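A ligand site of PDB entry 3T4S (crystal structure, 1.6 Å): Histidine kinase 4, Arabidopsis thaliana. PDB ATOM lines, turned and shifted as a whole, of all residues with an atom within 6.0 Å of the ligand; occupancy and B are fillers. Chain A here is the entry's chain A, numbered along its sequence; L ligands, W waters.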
ATOM      1  N   SER A  74       3.011  -4.602  11.774  1.00  0.00           N
ATOM      2  CA  SER A  74       1.930  -3.611  11.914  1.00  0.00           C
ATOM      3  C   SER A  74       0.910  -4.029  12.961  1.00  0.00           C
ATOM      4  O   SER A  74       0.131  -3.206  13.444  1.00  0.00           O
ATOM      5  CB  SER A  74       1.218  -3.388  10.608  1.00  0.00           C
ATOM      6  OG  SER A  74       0.707  -4.584  10.097  1.00  0.00           O
ATOM      7  N   GLY A  75       0.881  -5.323  13.294  1.00  0.00           N
ATOM      8  CA  GLY A  75      -0.071  -5.829  14.260  1.00  0.00           C
ATOM      9  C   GLY A  75       0.103  -7.319  14.460  1.00  0.00           C
ATOM     10  O   GLY A  75       0.714  -7.972  13.628  1.00  0.00           O
ATOM     11  N   VAL A  76      -0.411  -7.823  15.575  1.00  0.00           N
ATOM     12  CA  VAL A  76      -0.430  -9.260  15.872  1.00  0.00           C
ATOM     13  C   VAL A  76      -1.823  -9.650  16.297  1.00  0.00           C
ATOM     14  O   VAL A  76      -2.603  -8.816  16.772  1.00  0.00           O
ATOM     15  CB  VAL A  76       0.598  -9.621  16.944  1.00  0.00           C
ATOM     16  CG1 VAL A  76       2.029  -9.350  16.451  1.00  0.00           C
ATOM     17  CG2 VAL A  76       0.367  -8.812  18.237  1.00  0.00           C
ATOM     18  N   ALA A  77      -2.162 -10.935  16.121  1.00  0.00           N
ATOM     19  CA  ALA A  77      -3.448 -11.429  16.517  1.00  0.00           C
ATOM     20  C   ALA A  77      -3.344 -12.911  16.811  1.00  0.00           C
ATOM     21  O   ALA A  77      -2.448 -13.600  16.299  1.00  0.00           O
ATOM     22  CB  ALA A  77      -4.478 -11.219  15.380  1.00  0.00           C
ATOM     23  N   TYR A  78      -4.316 -13.411  17.558  1.00  0.00           N
ATOM     24  CA  TYR A  78      -4.374 -14.844  17.870  1.00  0.00           C
ATOM     25  C   TYR A  78      -5.674 -15.434  17.336  1.00  0.00           C
ATOM     26  O   TYR A  78      -6.784 -14.937  17.650  1.00  0.00           O
ATOM     27  CB  TYR A  78      -4.269 -15.102  19.370  1.00  0.00           C
ATOM     28  CG  TYR A  78      -4.391 -16.565  19.682  1.00  0.00           C
ATOM     29  CD1 TYR A  78      -3.370 -17.435  19.339  1.00  0.00           C
ATOM     30  CD2 TYR A  78      -5.553 -17.076  20.260  1.00  0.00           C
ATOM     31  CE1 TYR A  78      -3.487 -18.818  19.578  1.00  0.00           C
ATOM     32  CE2 TYR A  78      -5.676 -18.471  20.485  1.00  0.00           C
ATOM     33  CZ  TYR A  78      -4.647 -19.302  20.132  1.00  0.00           C
ATOM     34  OH  TYR A  78      -4.714 -20.687  20.323  1.00  0.00           O
ATOM     35  N   ALA A  79      -5.501 -16.478  16.496  1.00  0.00           N
ATOM     36  CA  ALA A  79      -6.604 -17.197  15.857  1.00  0.00           C
ATOM     37  C   ALA A  79      -6.720 -18.569  16.492  1.00  0.00           C
ATOM     38  O   ALA A  79      -5.727 -19.255  16.646  1.00  0.00           O
ATOM     39  CB  ALA A  79      -6.372 -17.314  14.359  1.00  0.00           C
ATOM     40  N   MET A 101     -12.603 -13.659   5.080  1.00  0.00           N
ATOM     41  CA  MET A 101     -11.767 -12.468   5.028  1.00  0.00           C
ATOM     42  C   MET A 101     -12.028 -11.630   3.782  1.00  0.00           C
ATOM     43  O   MET A 101     -11.814 -10.419   3.800  1.00  0.00           O
ATOM     44  CB  MET A 101     -10.288 -12.809   5.166  1.00  0.00           C
ATOM     45  CG  MET A 101      -9.679 -13.365   3.985  1.00  0.00           C
ATOM     46  SD  MET A 101      -7.899 -13.327   4.218  1.00  0.00           S
ATOM     47  CE  MET A 101      -7.762 -14.284   5.721  1.00  0.00           C
ATOM     48  N   VAL A 116     -10.001 -15.256  14.320  1.00  0.00           N
ATOM     49  CA  VAL A 116      -9.266 -14.387  15.233  1.00  0.00           C
ATOM     50  C   VAL A 116     -10.140 -14.064  16.442  1.00  0.00           C
ATOM     51  O   VAL A 116     -11.263 -13.519  16.287  1.00  0.00           O
ATOM     52  CB  VAL A 116      -8.776 -13.124  14.537  1.00  0.00           C
ATOM     53  CG1 VAL A 116      -8.146 -12.166  15.575  1.00  0.00           C
ATOM     54  CG2 VAL A 116      -7.719 -13.465  13.485  1.00  0.00           C
ATOM     55  N   VAL A 123      -4.869  -4.006  14.216  1.00  0.00           N
ATOM     56  CA  VAL A 123      -5.459  -4.937  13.261  1.00  0.00           C
ATOM     57  C   VAL A 123      -6.805  -5.460  13.794  1.00  0.00           C
ATOM     58  O   VAL A 123      -7.149  -6.633  13.634  1.00  0.00           O
ATOM     59  CB  VAL A 123      -4.506  -6.098  12.921  1.00  0.00           C
ATOM     60  CG1 VAL A 123      -3.301  -5.578  12.148  1.00  0.00           C
ATOM     61  CG2 VAL A 123      -4.043  -6.846  14.179  1.00  0.00           C
ATOM     62  N   TYR A 125      -9.734  -5.114  12.734  1.00  0.00           N
ATOM     63  CA  TYR A 125     -10.609  -5.598  11.649  1.00  0.00           C
ATOM     64  C   TYR A 125     -10.438  -7.095  11.424  1.00  0.00           C
ATOM     65  O   TYR A 125     -11.275  -7.709  10.756  1.00  0.00           O
ATOM     66  CB  TYR A 125     -10.363  -4.858  10.328  1.00  0.00           C
ATOM     67  CG  TYR A 125      -8.899  -4.703  10.004  1.00  0.00           C
ATOM     68  CD1 TYR A 125      -8.160  -5.736   9.412  1.00  0.00           C
ATOM     69  CD2 TYR A 125      -8.228  -3.520  10.313  1.00  0.00           C
ATOM     70  CE1 TYR A 125      -6.786  -5.582   9.130  1.00  0.00           C
ATOM     71  CE2 TYR A 125      -6.876  -3.359  10.033  1.00  0.00           C
ATOM     72  CZ  TYR A 125      -6.170  -4.382   9.449  1.00  0.00           C
ATOM     73  OH  TYR A 125      -4.843  -4.165   9.189  1.00  0.00           O
ATOM     74  N   LEU A 126      -9.393  -7.703  11.989  1.00  0.00           N
ATOM     75  CA  LEU A 126      -9.273  -9.156  11.902  1.00  0.00           C
ATOM     76  C   LEU A 126     -10.217  -9.921  12.824  1.00  0.00           C
ATOM     77  O   LEU A 126     -10.453 -11.107  12.612  1.00  0.00           O
ATOM     78  CB  LEU A 126      -7.861  -9.597  12.240  1.00  0.00           C
ATOM     79  CG  LEU A 126      -6.706  -9.123  11.362  1.00  0.00           C
ATOM     80  CD1 LEU A 126      -5.344  -9.597  11.948  1.00  0.00           C
ATOM     81  CD2 LEU A 126      -6.872  -9.573   9.885  1.00  0.00           C
ATOM     82  N   MET A 131      -8.913 -17.011   9.404  1.00  0.00           N
ATOM     83  CA  MET A 131      -7.655 -16.784   8.720  1.00  0.00           C
ATOM     84  C   MET A 131      -7.343 -17.907   7.702  1.00  0.00           C
ATOM     85  O   MET A 131      -6.481 -17.752   6.841  1.00  0.00           O
ATOM     86  CB  MET A 131      -6.520 -16.526   9.713  1.00  0.00           C
ATOM     87  CG  MET A 131      -6.803 -15.304  10.631  1.00  0.00           C
ATOM     88  SD  MET A 131      -7.274 -13.829   9.783  1.00  0.00           S
ATOM     89  CE  MET A 131      -5.748 -13.473   8.880  1.00  0.00           C
ATOM     90  N   ASP A 137      -2.524 -17.028   4.167  1.00  0.00           N
ATOM     91  CA  ASP A 137      -2.667 -17.307   5.590  1.00  0.00           C
ATOM     92  C   ASP A 137      -2.928 -18.783   5.835  1.00  0.00           C
ATOM     93  O   ASP A 137      -2.375 -19.362   6.767  1.00  0.00           O
ATOM     94  CB  ASP A 137      -3.777 -16.439   6.170  1.00  0.00           C
ATOM     95  CG  ASP A 137      -3.288 -15.026   6.489  1.00  0.00           C
ATOM     96  OD1 ASP A 137      -2.619 -14.866   7.541  1.00  0.00           O
ATOM     97  OD2 ASP A 137      -3.613 -14.119   5.716  1.00  0.00           O
ATOM     98  N   ILE A 141      -0.680 -21.261   8.121  1.00  0.00           N
ATOM     99  CA  ILE A 141      -1.238 -21.932   9.288  1.00  0.00           C
ATOM    100  C   ILE A 141      -0.898 -23.420   9.256  1.00  0.00           C
ATOM    101  O   ILE A 141      -0.436 -23.974  10.263  1.00  0.00           O
ATOM    102  CB  ILE A 141      -2.762 -21.680   9.345  1.00  0.00           C
ATOM    103  CG1 ILE A 141      -2.971 -20.277   9.934  1.00  0.00           C
ATOM    104  CG2 ILE A 141      -3.478 -22.764  10.158  1.00  0.00           C
ATOM    105  CD1 ILE A 141      -4.371 -19.704   9.714  1.00  0.00           C
ATOM    106  N   PHE A 156       2.358 -10.585  -0.393  1.00  0.00           N
ATOM    107  CA  PHE A 156       1.016 -10.321  -0.904  1.00  0.00           C
ATOM    108  C   PHE A 156       0.425  -9.065  -0.280  1.00  0.00           C
ATOM    109  O   PHE A 156       0.986  -8.531   0.695  1.00  0.00           O
ATOM    110  CB  PHE A 156       0.090 -11.548  -0.669  1.00  0.00           C
ATOM    111  CG  PHE A 156      -0.310 -11.784   0.764  1.00  0.00           C
ATOM    112  CD1 PHE A 156       0.589 -12.298   1.691  1.00  0.00           C
ATOM    113  CD2 PHE A 156      -1.614 -11.561   1.165  1.00  0.00           C
ATOM    114  CE1 PHE A 156       0.214 -12.530   2.983  1.00  0.00           C
ATOM    115  CE2 PHE A 156      -1.988 -11.812   2.444  1.00  0.00           C
ATOM    116  CZ  PHE A 156      -1.092 -12.286   3.353  1.00  0.00           C
ATOM    117  N   ARG A 157      -0.688  -8.584  -0.830  1.00  0.00           N
ATOM    118  CA  ARG A 157      -1.316  -7.375  -0.316  1.00  0.00           C
ATOM    119  C   ARG A 157      -2.233  -7.701   0.884  1.00  0.00           C
ATOM    120  O   ARG A 157      -3.187  -8.499   0.805  1.00  0.00           O
ATOM    121  CB  ARG A 157      -2.014  -6.543  -1.414  1.00  0.00           C
ATOM    122  CG  ARG A 157      -0.993  -5.982  -2.417  1.00  0.00           C
ATOM    123  CD  ARG A 157      -1.507  -4.879  -3.315  1.00  0.00           C
ATOM    124  NE  ARG A 157      -0.419  -4.344  -4.146  1.00  0.00           N
ATOM    125  CZ  ARG A 157       0.491  -3.440  -3.761  1.00  0.00           C
ATOM    126  NH1 ARG A 157       0.471  -2.909  -2.533  1.00  0.00           N
ATOM    127  NH2 ARG A 157       1.442  -3.047  -4.616  1.00  0.00           N
ATOM    128  N   LEU A 158      -1.888  -7.079   2.007  1.00  0.00           N
ATOM    129  CA  LEU A 158      -2.539  -7.304   3.265  1.00  0.00           C
ATOM    130  C   LEU A 158      -3.951  -6.724   3.324  1.00  0.00           C
ATOM    131  O   LEU A 158      -4.307  -5.812   2.588  1.00  0.00           O
ATOM    132  CB  LEU A 158      -1.673  -6.734   4.404  1.00  0.00           C
ATOM    133  CG  LEU A 158      -0.265  -7.317   4.504  1.00  0.00           C
ATOM    134  CD1 LEU A 158       0.560  -6.470   5.507  1.00  0.00           C
ATOM    135  CD2 LEU A 158      -0.262  -8.803   4.875  1.00  0.00           C
ATOM    136  N   LEU A 159      -4.765  -7.284   4.190  1.00  0.00           N
ATOM    137  CA  LEU A 159      -6.113  -6.800   4.414  1.00  0.00           C
ATOM    138  C   LEU A 159      -6.130  -5.355   4.851  1.00  0.00           C
ATOM    139  O   LEU A 159      -5.234  -4.919   5.591  1.00  0.00           O
ATOM    140  CB  LEU A 159      -6.818  -7.648   5.479  1.00  0.00           C
ATOM    141  CG  LEU A 159      -7.186  -9.054   5.071  1.00  0.00           C
ATOM    142  CD1 LEU A 159      -7.559  -9.835   6.346  1.00  0.00           C
ATOM    143  CD2 LEU A 159      -8.319  -9.048   4.045  1.00  0.00           C
ATOM    144  N   VAL A 167       3.159 -12.376   5.965  1.00  0.00           N
ATOM    145  CA  VAL A 167       2.632 -12.759   7.260  1.00  0.00           C
ATOM    146  C   VAL A 167       3.547 -13.803   7.912  1.00  0.00           C
ATOM    147  O   VAL A 167       4.047 -14.701   7.243  1.00  0.00           O
ATOM    148  CB  VAL A 167       1.184 -13.290   7.134  1.00  0.00           C
ATOM    149  CG1 VAL A 167       0.737 -13.965   8.422  1.00  0.00           C
ATOM    150  CG2 VAL A 167       0.261 -12.125   6.802  1.00  0.00           C
ATOM    151  N   LEU A 168       3.738 -13.630   9.225  1.00  0.00           N
ATOM    152  CA  LEU A 168       4.499 -14.521  10.094  1.00  0.00           C
ATOM    153  C   LEU A 168       3.477 -15.250  10.977  1.00  0.00           C
ATOM    154  O   LEU A 168       2.625 -14.591  11.579  1.00  0.00           O
ATOM    155  CB  LEU A 168       5.428 -13.699  10.974  1.00  0.00           C
ATOM    156  CG  LEU A 168       6.065 -14.403  12.156  1.00  0.00           C
ATOM    157  CD1 LEU A 168       7.145 -15.352  11.687  1.00  0.00           C
ATOM    158  CD2 LEU A 168       6.660 -13.377  13.138  1.00  0.00           C
ATOM    159  N   THR A 169       3.534 -16.574  11.032  1.00  0.00           N
ATOM    160  CA  THR A 169       2.590 -17.345  11.832  1.00  0.00           C
ATOM    161  C   THR A 169       3.364 -18.366  12.694  1.00  0.00           C
ATOM    162  O   THR A 169       4.282 -19.027  12.190  1.00  0.00           O
ATOM    163  CB  THR A 169       1.556 -18.035  10.914  1.00  0.00           C
ATOM    164  OG1 THR A 169       0.930 -17.071  10.061  1.00  0.00           O
ATOM    165  CG2 THR A 169       0.495 -18.767  11.776  1.00  0.00           C
ATOM    166  N   TYR A 193      -3.075 -20.207  16.427  1.00  0.00           N
ATOM    167  CA  TYR A 193      -2.038 -19.612  15.625  1.00  0.00           C
ATOM    168  C   TYR A 193      -1.860 -18.159  15.995  1.00  0.00           C
ATOM    169  O   TYR A 193      -2.809 -17.389  16.043  1.00  0.00           O
ATOM    170  CB  TYR A 193      -2.392 -19.746  14.142  1.00  0.00           C
ATOM    171  CG  TYR A 193      -3.116 -21.059  13.830  1.00  0.00           C
ATOM    172  CD1 TYR A 193      -2.385 -22.240  13.677  1.00  0.00           C
ATOM    173  CD2 TYR A 193      -4.512 -21.105  13.722  1.00  0.00           C
ATOM    174  CE1 TYR A 193      -3.057 -23.416  13.446  1.00  0.00           C
ATOM    175  CE2 TYR A 193      -5.170 -22.266  13.486  1.00  0.00           C
ATOM    176  CZ  TYR A 193      -4.416 -23.429  13.349  1.00  0.00           C
ATOM    177  OH  TYR A 193      -5.083 -24.626  13.079  1.00  0.00           O
ATOM    178  N   LEU A 194      -0.625 -17.781  16.308  1.00  0.00           N
ATOM    179  CA  LEU A 194      -0.290 -16.407  16.634  1.00  0.00           C
ATOM    180  C   LEU A 194       0.375 -15.829  15.372  1.00  0.00           C
ATOM    181  O   LEU A 194       1.416 -16.337  14.932  1.00  0.00           O
ATOM    182  CB  LEU A 194       0.656 -16.360  17.838  1.00  0.00           C
ATOM    183  CG  LEU A 194       0.863 -15.056  18.603  1.00  0.00           C
ATOM    184  CD1 LEU A 194       1.168 -13.836  17.720  1.00  0.00           C
ATOM    185  CD2 LEU A 194      -0.356 -14.740  19.485  1.00  0.00           C
ATOM    186  N   GLY A 195      -0.245 -14.826  14.776  1.00  0.00           N
ATOM    187  CA  GLY A 195       0.213 -14.261  13.509  1.00  0.00           C
ATOM    188  C   GLY A 195       0.500 -12.786  13.628  1.00  0.00           C
ATOM    189  O   GLY A 195      -0.033 -12.096  14.477  1.00  0.00           O
ATOM    190  N   GLY A 196       1.397 -12.330  12.772  1.00  0.00           N
ATOM    191  CA  GLY A 196       1.797 -10.948  12.712  1.00  0.00           C
ATOM    192  C   GLY A 196       2.011 -10.560  11.261  1.00  0.00           C
ATOM    193  O   GLY A 196       2.431 -11.396  10.436  1.00  0.00           O
ATOM    194  N   ALA A 197       1.647  -9.321  10.945  1.00  0.00           N
ATOM    195  CA  ALA A 197       1.758  -8.782   9.606  1.00  0.00           C
ATOM    196  C   ALA A 197       3.036  -7.937   9.498  1.00  0.00           C
ATOM    197  O   ALA A 197       3.154  -6.922  10.190  1.00  0.00           O
ATOM    198  CB  ALA A 197       0.581  -7.895   9.322  1.00  0.00           C
HETATM  199  C1  LIG L   1      -3.204 -14.025  12.555  1.00  0.00           C
HETATM  200  C2  LIG L   1      -3.403 -15.357  12.761  1.00  0.00           C
HETATM  201  C3  LIG L   1      -2.843 -16.052  11.737  1.00  0.00           C
HETATM  202  O1  LIG L   1      -2.262 -15.103  10.864  1.00  0.00           O
HETATM  203  C4  LIG L   1      -2.587 -13.874  11.349  1.00  0.00           C
HETATM  204  C5  LIG L   1      -2.029 -12.606  10.714  1.00  0.00           C
HETATM  205  N1  LIG L   1      -2.502 -12.411   9.366  1.00  0.00           N
HETATM  206  C6  LIG L   1      -2.723 -11.127   8.890  1.00  0.00           C
HETATM  207  N2  LIG L   1      -2.534 -10.095   9.772  1.00  0.00           N
HETATM  208  C7  LIG L   1      -2.775  -8.834   9.353  1.00  0.00           C
HETATM  209  N3  LIG L   1      -3.172  -8.542   8.124  1.00  0.00           N
HETATM  210  C8  LIG L   1      -3.419  -9.489   7.223  1.00  0.00           C
HETATM  211  C9  LIG L   1      -3.173 -10.853   7.603  1.00  0.00           C
HETATM  212  N4  LIG L   1      -3.462 -11.620   6.468  1.00  0.00           N
HETATM  213  C10 LIG L   1      -3.857 -10.756   5.470  1.00  0.00           C
HETATM  214  N5  LIG L   1      -3.828  -9.486   5.940  1.00  0.00           N
HETATM  215  O   HOH W   1      -3.617  -5.839   7.519  1.00  0.00           O
HETATM  216  O   HOH W   2      -1.502 -17.199   8.723  1.00  0.00           O
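OD2 of Asp 137 is in hydrogen-bond range of N4 of the ligand (2.6 Å).
A nitrogen (N5) of the ligand lies close to the backbone NH (N) of Leu 159 (3.0 Å).
The backbone NH (N) of Ala 197 sits at hydrogen-bond distance from the backbone carbonyl oxygen (O) of Gly 75 (3.1 Å).
The backbone carbonyl oxygen (O) of Gly 195 sits at hydrogen-bond distance from the backbone NH (N) of Ala 77, 2.9 Å away.
The backbone NH (N) of Tyr 193 sits at hydrogen-bond distance from the backbone carbonyl oxygen (O) of Ala 79, at 2.8 Å.
The backbone NH (N) of Ser 74 sits at hydrogen-bond distance from the backbone carbonyl oxygen (O) of Ala 197 (2.8 Å).
O of Ala 77 touches C1 of the ligand, at 3.8 Å.
Ala 79 touches the ligand (CB to C2, 3.9 Å).
Leu 126 touches the ligand.
Met 131 touches the ligand (CE to N1, 3.4 Å).
CE2 of Phe 156 touches C10 of the ligand, 3.7 Å away.
Leu 158 touches the ligand.
CG1 of Val 167 touches N1 of the ligand, at 3.7 Å.
Thr 169 touches the ligand (OG1 to O1, 3.8 Å).
Tyr 193 touches the ligand.
Gly 195 touches the ligand.
Ala 197 touches the ligand (CB to C7, 3.5 Å).
Hydrophobic or aromatic side chains that line the ligand: Ala 79, Leu 126, Met 131, Phe 156, Leu 158, Leu 159, Val 167 and Ala 197.
The nearest printed residue that does not touch the ligand is Gly 196 (4.01 Å).
Water W1 lies within hydrogen-bond range of OH of Tyr 125 (2.7 Å) and O of Leu 159 (2.7 Å).
Water W2 lies within hydrogen-bond range of the side-chain hydroxyl (OG1) of Thr 169 (2.8 Å), the side-chain carboxylate (OD1) of Asp 137 (2.8 Å) and an oxygen (O1) of the ligand (3.1 Å).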
